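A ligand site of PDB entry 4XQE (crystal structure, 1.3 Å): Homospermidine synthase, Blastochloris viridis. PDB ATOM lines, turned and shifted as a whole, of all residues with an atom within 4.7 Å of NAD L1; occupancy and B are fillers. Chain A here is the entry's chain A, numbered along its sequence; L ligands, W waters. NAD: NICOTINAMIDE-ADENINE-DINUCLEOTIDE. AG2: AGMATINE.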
ATOM      1  N   ILE A  15      28.708  20.412 -28.549  1.00  0.00           N
ATOM      2  CA  ILE A  15      28.932  19.483 -27.447  1.00  0.00           C
ATOM      3  C   ILE A  15      27.728  19.628 -26.566  1.00  0.00           C
ATOM      4  O   ILE A  15      27.481  20.685 -25.994  1.00  0.00           O
ATOM      5  CB  ILE A  15      30.218  19.812 -26.671  1.00  0.00           C
ATOM      6  CG1 ILE A  15      31.418  19.875 -27.634  1.00  0.00           C
ATOM      7  CG2 ILE A  15      30.458  18.789 -25.564  1.00  0.00           C
ATOM      8  CD1 ILE A  15      32.690  20.347 -26.969  1.00  0.00           C
ATOM      9  N   GLY A  16      26.956  18.557 -26.488  1.00  0.00           N
ATOM     10  CA  GLY A  16      25.721  18.545 -25.724  1.00  0.00           C
ATOM     11  C   GLY A  16      24.485  18.811 -26.556  1.00  0.00           C
ATOM     12  O   GLY A  16      24.417  19.773 -27.321  1.00  0.00           O
ATOM     13  N   PHE A  17      23.480  17.969 -26.359  1.00  0.00           N
ATOM     14  CA  PHE A  17      22.235  18.056 -27.125  1.00  0.00           C
ATOM     15  C   PHE A  17      21.071  17.791 -26.187  1.00  0.00           C
ATOM     16  O   PHE A  17      20.224  16.947 -26.440  1.00  0.00           O
ATOM     17  CB  PHE A  17      22.250  17.092 -28.311  1.00  0.00           C
ATOM     18  CG  PHE A  17      21.252  17.429 -29.383  1.00  0.00           C
ATOM     19  CD1 PHE A  17      21.298  18.646 -30.024  1.00  0.00           C
ATOM     20  CD2 PHE A  17      20.304  16.509 -29.766  1.00  0.00           C
ATOM     21  CE1 PHE A  17      20.393  18.950 -31.020  1.00  0.00           C
ATOM     22  CE2 PHE A  17      19.399  16.813 -30.762  1.00  0.00           C
ATOM     23  CZ  PHE A  17      19.445  18.039 -31.399  1.00  0.00           C
ATOM     24  N   GLY A  18      21.061  18.564 -25.092  1.00  0.00           N
ATOM     25  CA  GLY A  18      19.958  18.550 -24.156  1.00  0.00           C
ATOM     26  C   GLY A  18      19.021  19.683 -24.522  1.00  0.00           C
ATOM     27  O   GLY A  18      18.906  20.045 -25.703  1.00  0.00           O
ATOM     28  N   SER A  19      18.369  20.285 -23.519  1.00  0.00           N
ATOM     29  CA  SER A  19      17.330  21.272 -23.813  1.00  0.00           C
ATOM     30  C   SER A  19      17.885  22.474 -24.610  1.00  0.00           C
ATOM     31  O   SER A  19      17.245  22.948 -25.565  1.00  0.00           O
ATOM     32  CB  SER A  19      16.568  21.712 -22.549  1.00  0.00           C
ATOM     33  OG  SER A  19      17.155  22.828 -21.915  1.00  0.00           O
ATOM     34  N   ILE A  20      19.090  22.927 -24.289  1.00  0.00           N
ATOM     35  CA  ILE A  20      19.619  24.105 -24.968  1.00  0.00           C
ATOM     36  C   ILE A  20      20.188  23.755 -26.346  1.00  0.00           C
ATOM     37  O   ILE A  20      19.971  24.477 -27.308  1.00  0.00           O
ATOM     38  CB  ILE A  20      20.646  24.844 -24.111  1.00  0.00           C
ATOM     39  CG1 ILE A  20      20.025  25.239 -22.760  1.00  0.00           C
ATOM     40  CG2 ILE A  20      21.164  26.080 -24.851  1.00  0.00           C
ATOM     41  CD1 ILE A  20      18.726  25.979 -22.837  1.00  0.00           C
ATOM     42  N   GLY A  21      20.936  22.659 -26.446  1.00  0.00           N
ATOM     43  CA  GLY A  21      21.410  22.228 -27.744  1.00  0.00           C
ATOM     44  C   GLY A  21      20.279  22.019 -28.737  1.00  0.00           C
ATOM     45  O   GLY A  21      20.383  22.361 -29.921  1.00  0.00           O
ATOM     46  N   ARG A  22      19.184  21.443 -28.254  1.00  0.00           N
ATOM     47  CA  ARG A  22      18.052  21.155 -29.131  1.00  0.00           C
ATOM     48  C   ARG A  22      17.414  22.441 -29.625  1.00  0.00           C
ATOM     49  O   ARG A  22      16.917  22.487 -30.755  1.00  0.00           O
ATOM     50  CB  ARG A  22      16.992  20.292 -28.442  1.00  0.00           C
ATOM     51  CG  ARG A  22      17.474  18.885 -28.213  1.00  0.00           C
ATOM     52  CD  ARG A  22      16.626  18.116 -27.201  1.00  0.00           C
ATOM     53  NE  ARG A  22      17.457  17.071 -26.624  1.00  0.00           N
ATOM     54  CZ  ARG A  22      17.038  16.095 -25.812  1.00  0.00           C
ATOM     55  NH1 ARG A  22      15.757  16.009 -25.453  1.00  0.00           N
ATOM     56  NH2 ARG A  22      17.936  15.211 -25.382  1.00  0.00           N
ATOM     57  N   ILE A  42      27.857  16.027 -30.324  1.00  0.00           N
ATOM     58  CA  ILE A  42      28.496  15.042 -29.445  1.00  0.00           C
ATOM     59  C   ILE A  42      27.740  15.027 -28.134  1.00  0.00           C
ATOM     60  O   ILE A  42      27.661  16.048 -27.445  1.00  0.00           O
ATOM     61  CB  ILE A  42      29.983  15.364 -29.163  1.00  0.00           C
ATOM     62  CG1 ILE A  42      30.761  15.599 -30.451  1.00  0.00           C
ATOM     63  CG2 ILE A  42      30.652  14.251 -28.340  1.00  0.00           C
ATOM     64  CD1 ILE A  42      32.159  16.116 -30.224  1.00  0.00           C
ATOM     65  N   ASP A  43      27.163  13.873 -27.771  1.00  0.00           N
ATOM     66  CA  ASP A  43      26.422  13.741 -26.516  1.00  0.00           C
ATOM     67  C   ASP A  43      26.322  12.254 -26.223  1.00  0.00           C
ATOM     68  O   ASP A  43      26.041  11.487 -27.123  1.00  0.00           O
ATOM     69  CB  ASP A  43      25.019  14.366 -26.695  1.00  0.00           C
ATOM     70  CG  ASP A  43      24.241  14.512 -25.386  1.00  0.00           C
ATOM     71  OD1 ASP A  43      24.046  13.516 -24.676  1.00  0.00           O
ATOM     72  OD2 ASP A  43      23.792  15.645 -25.088  1.00  0.00           O
ATOM     73  N   PRO A  44      26.534  11.855 -24.957  1.00  0.00           N
ATOM     74  CA  PRO A  44      26.489  10.436 -24.591  1.00  0.00           C
ATOM     75  C   PRO A  44      25.075   9.839 -24.518  1.00  0.00           C
ATOM     76  O   PRO A  44      24.964   8.614 -24.443  1.00  0.00           O
ATOM     77  CB  PRO A  44      27.109  10.402 -23.192  1.00  0.00           C
ATOM     78  CG  PRO A  44      26.854  11.753 -22.631  1.00  0.00           C
ATOM     79  CD  PRO A  44      26.945  12.698 -23.818  1.00  0.00           C
ATOM     80  N   SER A  45      24.036  10.665 -24.572  1.00  0.00           N
ATOM     81  CA  SER A  45      22.658  10.206 -24.309  1.00  0.00           C
ATOM     82  C   SER A  45      22.011   9.508 -25.504  1.00  0.00           C
ATOM     83  O   SER A  45      22.092   9.975 -26.649  1.00  0.00           O
ATOM     84  CB  SER A  45      21.802  11.414 -23.901  1.00  0.00           C
ATOM     85  OG  SER A  45      20.431  11.177 -24.065  1.00  0.00           O
ATOM     86  N   GLN A  62      29.126   9.981 -27.375  1.00  0.00           N
ATOM     87  CA  GLN A  62      30.330   9.881 -26.574  1.00  0.00           C
ATOM     88  C   GLN A  62      30.333  10.981 -25.542  1.00  0.00           C
ATOM     89  O   GLN A  62      29.989  12.114 -25.851  1.00  0.00           O
ATOM     90  CB  GLN A  62      31.557  10.013 -27.488  1.00  0.00           C
ATOM     91  CG  GLN A  62      32.879   9.811 -26.790  1.00  0.00           C
ATOM     92  CD  GLN A  62      32.994   8.450 -26.170  1.00  0.00           C
ATOM     93  OE1 GLN A  62      33.397   8.314 -25.001  1.00  0.00           O
ATOM     94  NE2 GLN A  62      32.629   7.425 -26.919  1.00  0.00           N
ATOM     95  N   ALA A  63      30.689  10.644 -24.314  1.00  0.00           N
ATOM     96  CA  ALA A  63      30.942  11.669 -23.303  1.00  0.00           C
ATOM     97  C   ALA A  63      32.330  12.248 -23.531  1.00  0.00           C
ATOM     98  O   ALA A  63      33.302  11.507 -23.681  1.00  0.00           O
ATOM     99  CB  ALA A  63      30.880  11.083 -21.927  1.00  0.00           C
ATOM    100  N   VAL A  64      32.414  13.574 -23.566  1.00  0.00           N
ATOM    101  CA  VAL A  64      33.702  14.248 -23.595  1.00  0.00           C
ATOM    102  C   VAL A  64      34.250  14.255 -22.182  1.00  0.00           C
ATOM    103  O   VAL A  64      33.570  14.689 -21.255  1.00  0.00           O
ATOM    104  CB  VAL A  64      33.542  15.691 -24.105  1.00  0.00           C
ATOM    105  CG1 VAL A  64      34.867  16.396 -24.121  1.00  0.00           C
ATOM    106  CG2 VAL A  64      32.907  15.679 -25.485  1.00  0.00           C
ATOM    107  N   LEU A  89      27.384  23.247 -25.028  1.00  0.00           N
ATOM    108  CA  LEU A  89      26.085  23.325 -24.372  1.00  0.00           C
ATOM    109  C   LEU A  89      25.866  22.090 -23.513  1.00  0.00           C
ATOM    110  O   LEU A  89      24.803  21.491 -23.489  1.00  0.00           O
ATOM    111  CB  LEU A  89      24.970  23.455 -25.409  1.00  0.00           C
ATOM    112  CG  LEU A  89      25.122  24.672 -26.333  1.00  0.00           C
ATOM    113  CD1 LEU A  89      24.121  24.667 -27.476  1.00  0.00           C
ATOM    114  CD2 LEU A  89      25.037  25.989 -25.535  1.00  0.00           C
ATOM    115  N   SER A  90      26.907  21.703 -22.809  1.00  0.00           N
ATOM    116  CA  SER A  90      26.933  20.443 -22.100  1.00  0.00           C
ATOM    117  C   SER A  90      26.933  20.635 -20.593  1.00  0.00           C
ATOM    118  O   SER A  90      27.000  21.774 -20.082  1.00  0.00           O
ATOM    119  CB  SER A  90      28.180  19.651 -22.509  1.00  0.00           C
ATOM    120  OG  SER A  90      29.379  20.347 -22.130  1.00  0.00           O
ATOM    121  N   VAL A  91      26.793  19.510 -19.889  1.00  0.00           N
ATOM    122  CA  VAL A  91      27.158  19.439 -18.478  1.00  0.00           C
ATOM    123  C   VAL A  91      28.370  18.512 -18.356  1.00  0.00           C
ATOM    124  O   VAL A  91      28.671  17.743 -19.279  1.00  0.00           O
ATOM    125  CB  VAL A  91      25.981  18.943 -17.584  1.00  0.00           C
ATOM    126  CG1 VAL A  91      24.834  19.932 -17.640  1.00  0.00           C
ATOM    127  CG2 VAL A  91      25.540  17.535 -17.963  1.00  0.00           C
ATOM    128  N   ASP A  92      29.057  18.610 -17.216  1.00  0.00           N
ATOM    129  CA  ASP A  92      30.096  17.652 -16.811  1.00  0.00           C
ATOM    130  C   ASP A  92      31.403  17.754 -17.617  1.00  0.00           C
ATOM    131  O   ASP A  92      32.242  16.849 -17.546  1.00  0.00           O
ATOM    132  CB  ASP A  92      29.584  16.207 -16.856  1.00  0.00           C
ATOM    133  CG  ASP A  92      28.447  15.944 -15.855  1.00  0.00           C
ATOM    134  OD1 ASP A  92      28.213  16.787 -14.968  1.00  0.00           O
ATOM    135  OD2 ASP A  92      27.813  14.869 -15.944  1.00  0.00           O
ATOM    136  N   THR A  93      31.562  18.832 -18.377  1.00  0.00           N
ATOM    137  CA  THR A  93      32.773  19.066 -19.170  1.00  0.00           C
ATOM    138  C   THR A  93      33.424  20.356 -18.723  1.00  0.00           C
ATOM    139  O   THR A  93      32.752  21.274 -18.278  1.00  0.00           O
ATOM    140  CB  THR A  93      32.434  19.213 -20.648  1.00  0.00           C
ATOM    141  OG1 THR A  93      31.553  20.332 -20.817  1.00  0.00           O
ATOM    142  CG2 THR A  93      31.736  17.969 -21.184  1.00  0.00           C
ATOM    143  N   THR A 112      27.741  28.654 -22.082  1.00  0.00           N
ATOM    144  CA  THR A 112      26.725  29.361 -21.295  1.00  0.00           C
ATOM    145  C   THR A 112      26.957  29.236 -19.798  1.00  0.00           C
ATOM    146  O   THR A 112      26.117  29.650 -19.009  1.00  0.00           O
ATOM    147  CB  THR A 112      25.302  28.816 -21.600  1.00  0.00           C
ATOM    148  OG1 THR A 112      25.171  27.474 -21.122  1.00  0.00           O
ATOM    149  CG2 THR A 112      24.999  28.885 -23.098  1.00  0.00           C
ATOM    150  N   VAL A 113      28.108  28.698 -19.435  1.00  0.00           N
ATOM    151  CA  VAL A 113      28.425  28.418 -18.053  1.00  0.00           C
ATOM    152  C   VAL A 113      29.912  28.088 -17.946  1.00  0.00           C
ATOM    153  O   VAL A 113      30.498  27.593 -18.927  1.00  0.00           O
ATOM    154  CB  VAL A 113      27.588  27.222 -17.546  1.00  0.00           C
ATOM    155  CG1 VAL A 113      27.905  25.950 -18.356  1.00  0.00           C
ATOM    156  CG2 VAL A 113      27.798  26.973 -16.057  1.00  0.00           C
ATOM    157  N   GLU A 115      31.739  25.477 -16.497  1.00  0.00           N
ATOM    158  CA  GLU A 115      31.480  24.154 -15.957  1.00  0.00           C
ATOM    159  C   GLU A 115      32.831  23.450 -15.690  1.00  0.00           C
ATOM    160  O   GLU A 115      33.783  23.653 -16.442  1.00  0.00           O
ATOM    161  CB  GLU A 115      30.672  23.343 -16.989  1.00  0.00           C
ATOM    162  CG  GLU A 115      30.227  21.937 -16.584  1.00  0.00           C
ATOM    163  CD  GLU A 115      28.995  21.913 -15.696  1.00  0.00           C
ATOM    164  OE1 GLU A 115      28.573  22.992 -15.197  1.00  0.00           O
ATOM    165  OE2 GLU A 115      28.454  20.793 -15.486  1.00  0.00           O
ATOM    166  N   GLY A 158      24.597  32.708 -22.331  1.00  0.00           N
ATOM    167  CA  GLY A 158      23.217  32.255 -22.424  1.00  0.00           C
ATOM    168  C   GLY A 158      22.261  33.381 -22.114  1.00  0.00           C
ATOM    169  O   GLY A 158      22.511  34.527 -22.468  1.00  0.00           O
ATOM    170  N   ALA A 159      21.134  33.045 -21.469  1.00  0.00           N
ATOM    171  CA  ALA A 159      20.190  34.073 -21.047  1.00  0.00           C
ATOM    172  C   ALA A 159      20.707  34.787 -19.803  1.00  0.00           C
ATOM    173  O   ALA A 159      20.685  36.010 -19.740  1.00  0.00           O
ATOM    174  CB  ALA A 159      18.863  33.445 -20.762  1.00  0.00           C
ATOM    175  N   ASN A 160      21.117  34.005 -18.820  1.00  0.00           N
ATOM    176  CA  ASN A 160      21.621  34.558 -17.582  1.00  0.00           C
ATOM    177  C   ASN A 160      22.476  33.483 -16.947  1.00  0.00           C
ATOM    178  O   ASN A 160      21.950  32.505 -16.416  1.00  0.00           O
ATOM    179  CB  ASN A 160      20.502  35.020 -16.629  1.00  0.00           C
ATOM    180  CG  ASN A 160      19.462  33.952 -16.308  1.00  0.00           C
ATOM    181  OD1 ASN A 160      18.839  33.357 -17.194  1.00  0.00           O
ATOM    182  ND2 ASN A 160      19.229  33.742 -15.037  1.00  0.00           N
ATOM    183  N   PRO A 161      23.804  33.606 -17.017  1.00  0.00           N
ATOM    184  CA  PRO A 161      24.576  34.724 -17.563  1.00  0.00           C
ATOM    185  C   PRO A 161      24.438  34.808 -19.072  1.00  0.00           C
ATOM    186  O   PRO A 161      24.171  33.802 -19.756  1.00  0.00           O
ATOM    187  CB  PRO A 161      26.016  34.324 -17.221  1.00  0.00           C
ATOM    188  CG  PRO A 161      25.973  32.806 -17.148  1.00  0.00           C
ATOM    189  CD  PRO A 161      24.658  32.529 -16.503  1.00  0.00           C
ATOM    190  N   TRP A 227      14.568  23.754 -17.798  1.00  0.00           N
ATOM    191  CA  TRP A 227      15.891  23.609 -18.392  1.00  0.00           C
ATOM    192  C   TRP A 227      16.631  22.603 -17.518  1.00  0.00           C
ATOM    193  O   TRP A 227      16.039  22.087 -16.573  1.00  0.00           O
ATOM    194  CB  TRP A 227      16.648  24.956 -18.451  1.00  0.00           C
ATOM    195  CG  TRP A 227      16.825  25.606 -17.101  1.00  0.00           C
ATOM    196  CD1 TRP A 227      15.896  26.287 -16.375  1.00  0.00           C
ATOM    197  CD2 TRP A 227      18.037  25.620 -16.316  1.00  0.00           C
ATOM    198  NE1 TRP A 227      16.447  26.708 -15.178  1.00  0.00           N
ATOM    199  CE2 TRP A 227      17.760  26.316 -15.140  1.00  0.00           C
ATOM    200  CE3 TRP A 227      19.317  25.116 -16.516  1.00  0.00           C
ATOM    201  CZ2 TRP A 227      18.727  26.532 -14.150  1.00  0.00           C
ATOM    202  CZ3 TRP A 227      20.284  25.332 -15.525  1.00  0.00           C
ATOM    203  CH2 TRP A 227      19.976  26.016 -14.355  1.00  0.00           C
ATOM    204  N   SER A 228      17.897  22.321 -17.823  1.00  0.00           N
ATOM    205  CA  SER A 228      18.671  21.307 -17.111  1.00  0.00           C
ATOM    206  C   SER A 228      18.282  21.073 -15.645  1.00  0.00           C
ATOM    207  O   SER A 228      18.405  21.958 -14.822  1.00  0.00           O
ATOM    208  CB  SER A 228      20.152  21.664 -17.133  1.00  0.00           C
ATOM    209  OG  SER A 228      20.938  20.543 -16.758  1.00  0.00           O
ATOM    210  N   VAL A 229      17.848  19.865 -15.321  1.00  0.00           N
ATOM    211  CA  VAL A 229      17.671  19.531 -13.922  1.00  0.00           C
ATOM    212  C   VAL A 229      19.031  19.287 -13.285  1.00  0.00           C
ATOM    213  O   VAL A 229      19.295  19.763 -12.182  1.00  0.00           O
ATOM    214  CB  VAL A 229      16.722  18.324 -13.723  1.00  0.00           C
ATOM    215  CG1 VAL A 229      16.723  17.826 -12.267  1.00  0.00           C
ATOM    216  CG2 VAL A 229      15.326  18.690 -14.137  1.00  0.00           C
ATOM    217  N   GLY A 231      21.899  20.477 -14.122  1.00  0.00           N
ATOM    218  CA  GLY A 231      22.545  21.771 -14.008  1.00  0.00           C
ATOM    219  C   GLY A 231      21.978  22.616 -12.887  1.00  0.00           C
ATOM    220  O   GLY A 231      22.712  23.242 -12.114  1.00  0.00           O
ATOM    221  N   GLU A 235      23.987  23.751  -9.449  1.00  0.00           N
ATOM    222  CA  GLU A 235      24.201  25.130  -9.065  1.00  0.00           C
ATOM    223  C   GLU A 235      23.422  25.473  -7.797  1.00  0.00           C
ATOM    224  O   GLU A 235      23.868  26.284  -7.001  1.00  0.00           O
ATOM    225  CB  GLU A 235      23.917  26.092 -10.197  1.00  0.00           C
ATOM    226  CG  GLU A 235      22.561  26.098 -10.660  1.00  0.00           C
ATOM    227  CD  GLU A 235      22.415  26.866 -11.951  1.00  0.00           C
ATOM    228  OE1 GLU A 235      23.344  26.821 -12.800  1.00  0.00           O
ATOM    229  OE2 GLU A 235      21.371  27.545 -12.093  1.00  0.00           O
ATOM    230  N   ILE A 348      12.543  17.480 -17.862  1.00  0.00           N
ATOM    231  CA  ILE A 348      12.511  18.846 -18.333  1.00  0.00           C
ATOM    232  C   ILE A 348      11.258  19.001 -19.180  1.00  0.00           C
ATOM    233  O   ILE A 348      11.000  18.217 -20.087  1.00  0.00           O
ATOM    234  CB  ILE A 348      13.765  19.162 -19.161  1.00  0.00           C
ATOM    235  CG1 ILE A 348      15.009  19.025 -18.288  1.00  0.00           C
ATOM    236  CG2 ILE A 348      13.662  20.567 -19.775  1.00  0.00           C
ATOM    237  CD1 ILE A 348      16.312  19.074 -19.084  1.00  0.00           C
ATOM    238  N   VAL A 398      17.772  31.406 -23.994  1.00  0.00           N
ATOM    239  CA  VAL A 398      19.139  30.952 -23.938  1.00  0.00           C
ATOM    240  C   VAL A 398      19.708  30.733 -25.344  1.00  0.00           C
ATOM    241  O   VAL A 398      20.790  31.247 -25.661  1.00  0.00           O
ATOM    242  CB  VAL A 398      19.286  29.660 -23.127  1.00  0.00           C
ATOM    243  CG1 VAL A 398      20.741  29.267 -23.040  1.00  0.00           C
ATOM    244  CG2 VAL A 398      18.696  29.832 -21.726  1.00  0.00           C
HETATM  245  PA  NAD L   1      20.446  19.272 -20.180  1.00  0.00           P
HETATM  246  O1A NAD L   1      20.601  18.626 -18.816  1.00  0.00           O
HETATM  247  O2A NAD L   1      19.111  19.250 -20.834  1.00  0.00           O
HETATM  248  O5B NAD L   1      21.470  18.613 -21.209  1.00  0.00           O
HETATM  249  C5B NAD L   1      22.830  18.382 -20.878  1.00  0.00           C
HETATM  250  C4B NAD L   1      23.322  17.540 -21.918  1.00  0.00           C
HETATM  251  O4B NAD L   1      24.774  17.305 -21.723  1.00  0.00           O
HETATM  252  C3B NAD L   1      22.847  16.046 -21.992  1.00  0.00           C
HETATM  253  O3B NAD L   1      21.979  15.759 -23.121  1.00  0.00           O
HETATM  254  C2B NAD L   1      23.642  15.223 -21.488  1.00  0.00           C
HETATM  255  O2B NAD L   1      23.730  13.889 -22.092  1.00  0.00           O
HETATM  256  C1B NAD L   1      24.991  16.042 -21.778  1.00  0.00           C
HETATM  257  N9A NAD L   1      26.242  15.557 -21.428  1.00  0.00           N
HETATM  258  C8A NAD L   1      26.455  15.032 -20.205  1.00  0.00           C
HETATM  259  N7A NAD L   1      27.714  14.702 -20.064  1.00  0.00           N
HETATM  260  C5A NAD L   1      28.360  15.031 -21.237  1.00  0.00           C
HETATM  261  C6A NAD L   1      29.706  14.937 -21.694  1.00  0.00           C
HETATM  262  N6A NAD L   1      30.700  14.384 -20.853  1.00  0.00           N
HETATM  263  N1A NAD L   1      29.984  15.331 -22.934  1.00  0.00           N
HETATM  264  C2A NAD L   1      29.061  15.828 -23.725  1.00  0.00           C
HETATM  265  N3A NAD L   1      27.799  15.980 -23.333  1.00  0.00           N
HETATM  266  C4A NAD L   1      27.414  15.578 -22.101  1.00  0.00           C
HETATM  267  O3  NAD L   1      20.996  20.750 -20.001  1.00  0.00           O
HETATM  268  PN  NAD L   1      20.594  22.080 -20.808  1.00  0.00           P
HETATM  269  O1N NAD L   1      20.678  21.831 -22.258  1.00  0.00           O
HETATM  270  O2N NAD L   1      19.266  22.620 -20.317  1.00  0.00           O
HETATM  271  O5D NAD L   1      21.792  23.041 -20.325  1.00  0.00           O
HETATM  272  C5D NAD L   1      23.048  22.860 -20.970  1.00  0.00           C
HETATM  273  C4D NAD L   1      24.090  23.739 -20.274  1.00  0.00           C
HETATM  274  O4D NAD L   1      23.745  24.983 -20.393  1.00  0.00           O
HETATM  275  C3D NAD L   1      24.189  23.414 -18.755  1.00  0.00           C
HETATM  276  O3D NAD L   1      25.476  23.402 -18.315  1.00  0.00           O
HETATM  277  C2D NAD L   1      23.653  24.668 -18.142  1.00  0.00           C
HETATM  278  O2D NAD L   1      23.804  24.803 -16.727  1.00  0.00           O
HETATM  279  C1D NAD L   1      23.700  25.672 -18.955  1.00  0.00           C
HETATM  280  N1N NAD L   1      22.651  26.623 -19.047  1.00  0.00           N
HETATM  281  C2N NAD L   1      22.972  27.949 -19.035  1.00  0.00           C
HETATM  282  C3N NAD L   1      21.958  28.891 -19.123  1.00  0.00           C
HETATM  283  C7N NAD L   1      22.186  30.396 -19.158  1.00  0.00           C
HETATM  284  O7N NAD L   1      21.247  31.151 -19.351  1.00  0.00           O
HETATM  285  N7N NAD L   1      23.501  30.873 -19.122  1.00  0.00           N
HETATM  286  C4N NAD L   1      20.644  28.484 -19.243  1.00  0.00           C
HETATM  287  C5N NAD L   1      20.370  27.119 -19.319  1.00  0.00           C
HETATM  288  C6N NAD L   1      21.411  26.215 -19.211  1.00  0.00           C
HETATM  289  N   AG2 L   2      16.711  31.634 -17.240  1.00  0.00           N
HETATM  290  CA  AG2 L   2      16.965  30.363 -16.606  1.00  0.00           C
HETATM  291  CB  AG2 L   2      18.426  29.939 -16.766  1.00  0.00           C
HETATM  292  CG  AG2 L   2      19.143  29.845 -15.427  1.00  0.00           C
HETATM  293  CD  AG2 L   2      20.624  29.469 -15.545  1.00  0.00           C
HETATM  294  NE  AG2 L   2      21.141  29.208 -14.236  1.00  0.00           N
HETATM  295  CZ  AG2 L   2      21.793  30.176 -13.430  1.00  0.00           C
HETATM  296  NH1 AG2 L   2      22.281  29.895 -12.132  1.00  0.00           N
HETATM  297  NH2 AG2 L   2      21.998  31.374 -13.822  1.00  0.00           N
HETATM  298  O   HOH W   1      24.784  14.005 -17.693  1.00  0.00           O
HETATM  299  O   HOH W   2      28.664  13.153 -17.915  1.00  0.00           O
HETATM  300  O   HOH W   3      17.686  17.123 -21.813  1.00  0.00           O
HETATM  301  O   HOH W   4      23.015  12.110 -20.320  1.00  0.00           O
HETATM  302  O   HOH W   5      31.305  12.617 -18.412  1.00  0.00           O
HETATM  303  O   HOH W   6      22.224  21.082 -24.342  1.00  0.00           O
HETATM  304  O   HOH W   7      19.089  17.654 -16.774  1.00  0.00           O
HETATM  305  O   HOH W   8      23.733  27.290 -15.584  1.00  0.00           O
HETATM  306  O   HOH W   9      21.806  16.068 -18.515  1.00  0.00           O
HETATM  307  O   HOH W  10      19.535  15.152 -22.632  1.00  0.00           O
HETATM  308  O   HOH W  11      25.820  23.390 -15.291  1.00  0.00           O
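The side-chain carboxylate of Asp 43 lies within hydrogen-bond range of an oxygen (O2B) of NAD L1, 2.6 Å away.
N of Ser 19 lies within hydrogen-bond range of O2A of NAD L1 (3.0 Å).
The side-chain hydroxyl (OG) of Ser 19 is in hydrogen-bond range of an oxygen (O2N) of NAD L1, at 2.7 Å.
An oxygen (O1N) of NAD L1 lies within hydrogen-bond range of the backbone NH (N) of Ile 20, at 2.8 Å.
N of Ser 228 sits at hydrogen-bond distance from O2N of NAD L1.
OG of Ser 228 is in hydrogen-bond range of O1A of NAD L1, at 2.8 Å.
The backbone NH (N) of Ala 159 lies within hydrogen-bond range of an oxygen (O7N) of NAD L1 (2.8 Å).
An oxygen (O3D) of NAD L1 sits at hydrogen-bond distance from the backbone carbonyl oxygen of Ser 90 (2.8 Å).
The backbone carbonyl oxygen (O) of Thr 112 lies within hydrogen-bond range of a nitrogen (N7N) of NAD L1 (2.9 Å).
The side-chain hydroxyl (OG1) of Thr 112 lies within hydrogen-bond range of an oxygen (O4D) of NAD L1 (3.0 Å).
N of Asn 160 is in hydrogen-bond range of O7N of NAD L1, 2.9 Å away.
N of Val 64 sits at hydrogen-bond distance from N1A of NAD L1.
The backbone carbonyl oxygen (O) of Val 64 sits at hydrogen-bond distance from a nitrogen (N6A) of NAD L1 (2.9 Å).
A nitrogen (N7N) of NAD L1 lies within hydrogen-bond range of the backbone carbonyl oxygen (O) of Pro 161 (3.1 Å).
O of Asn 160 sits at hydrogen-bond distance from NH2 of AG2 L2, at 2.8 Å.
N of AG2 L2 is in hydrogen-bond range of OD1 of Asn 160, 2.7 Å away.
OE2 of Glu 235 is in salt-bridge range of NH1 of AG2 L2.
The backbone carbonyl oxygen (O) of Val 91 sits close to a nitrogen (N7A) of NAD L1 (3.3 Å).
Merely in contact with NAD L1: Ile 348, Gly 18, Leu 89, Pro 44, Val 398, Ala 63, Val 113, Trp 227, Gly 158, Thr 93, Ser 45, Ile 15, Phe 17 and Ile 42.
25 residues have an atom within 4 Å of NAD L1: Ile 15, Phe 17, Gly 18, Ser 19, Ile 20, Ile 42, Asp 43, Pro 44, Ser 45, Ala 63, Val 64, Leu 89, Ser 90, Val 91, Thr 93, Thr 112, Val 113, Gly 158, Ala 159, Asn 160, Pro 161, Trp 227, Ser 228, Ile 348 and Val 398.
OD1 of Asp 43 sits at hydrogen-bond distance from N of Ser 45 (2.9 Å).
OD2 of Asp 43 lies within hydrogen-bond range of N of Phe 17, 2.7 Å away.
The backbone carbonyl oxygen (O) of Asp 43 sits at hydrogen-bond distance from the backbone NH (N) of Gln 62, 3.4 Å away.
The side-chain hydroxyl (OG) of Ser 228 sits at hydrogen-bond distance from the backbone NH (N) of Gly 231, 2.8 Å away.
The backbone NH of Ser 90 lies within hydrogen-bond range of the backbone carbonyl oxygen of Ile 15 (3.4 Å).
N of Leu 89 is in hydrogen-bond range of O of Ile 15, at 2.7 Å.
O of Phe 17 is in hydrogen-bond range of NE of Arg 22, 2.8 Å away.
The backbone carbonyl oxygen (O) of Ile 42 is in hydrogen-bond range of the backbone NH (N) of Gly 16 (2.8 Å).
Water W10 bridges an oxygen (O3B) of NAD L1 (2.6 Å) and the guanidinium group of Arg 22 (3.2 Å).
Water W6 lies within hydrogen-bond range of an oxygen (O1N) of NAD L1, the backbone carbonyl oxygen (O) of Leu 89, the backbone NH (N) of Gly 18 and the backbone NH (N) of Gly 21.
Water W7 lies within hydrogen-bond range of O1A of NAD L1 (2.7 Å), N of Val 229 (2.9 Å) and OG of Ser 228 (3.4 Å).
Water W8 lies within hydrogen-bond range of O2D of NAD L1 (2.7 Å), OE1 of Glu 235 (2.8 Å) and NE of AG2 L2 (3.5 Å).
Water W2 bridges the side-chain carboxylate of Asp 92 (2.7 Å) and a nitrogen (N7A) of NAD L1 (2.8 Å).
Water W11 lies within hydrogen-bond range of the side-chain carboxylate (OE1) of Glu 115 (2.8 Å) and an oxygen (O2D) of NAD L1 (2.9 Å).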
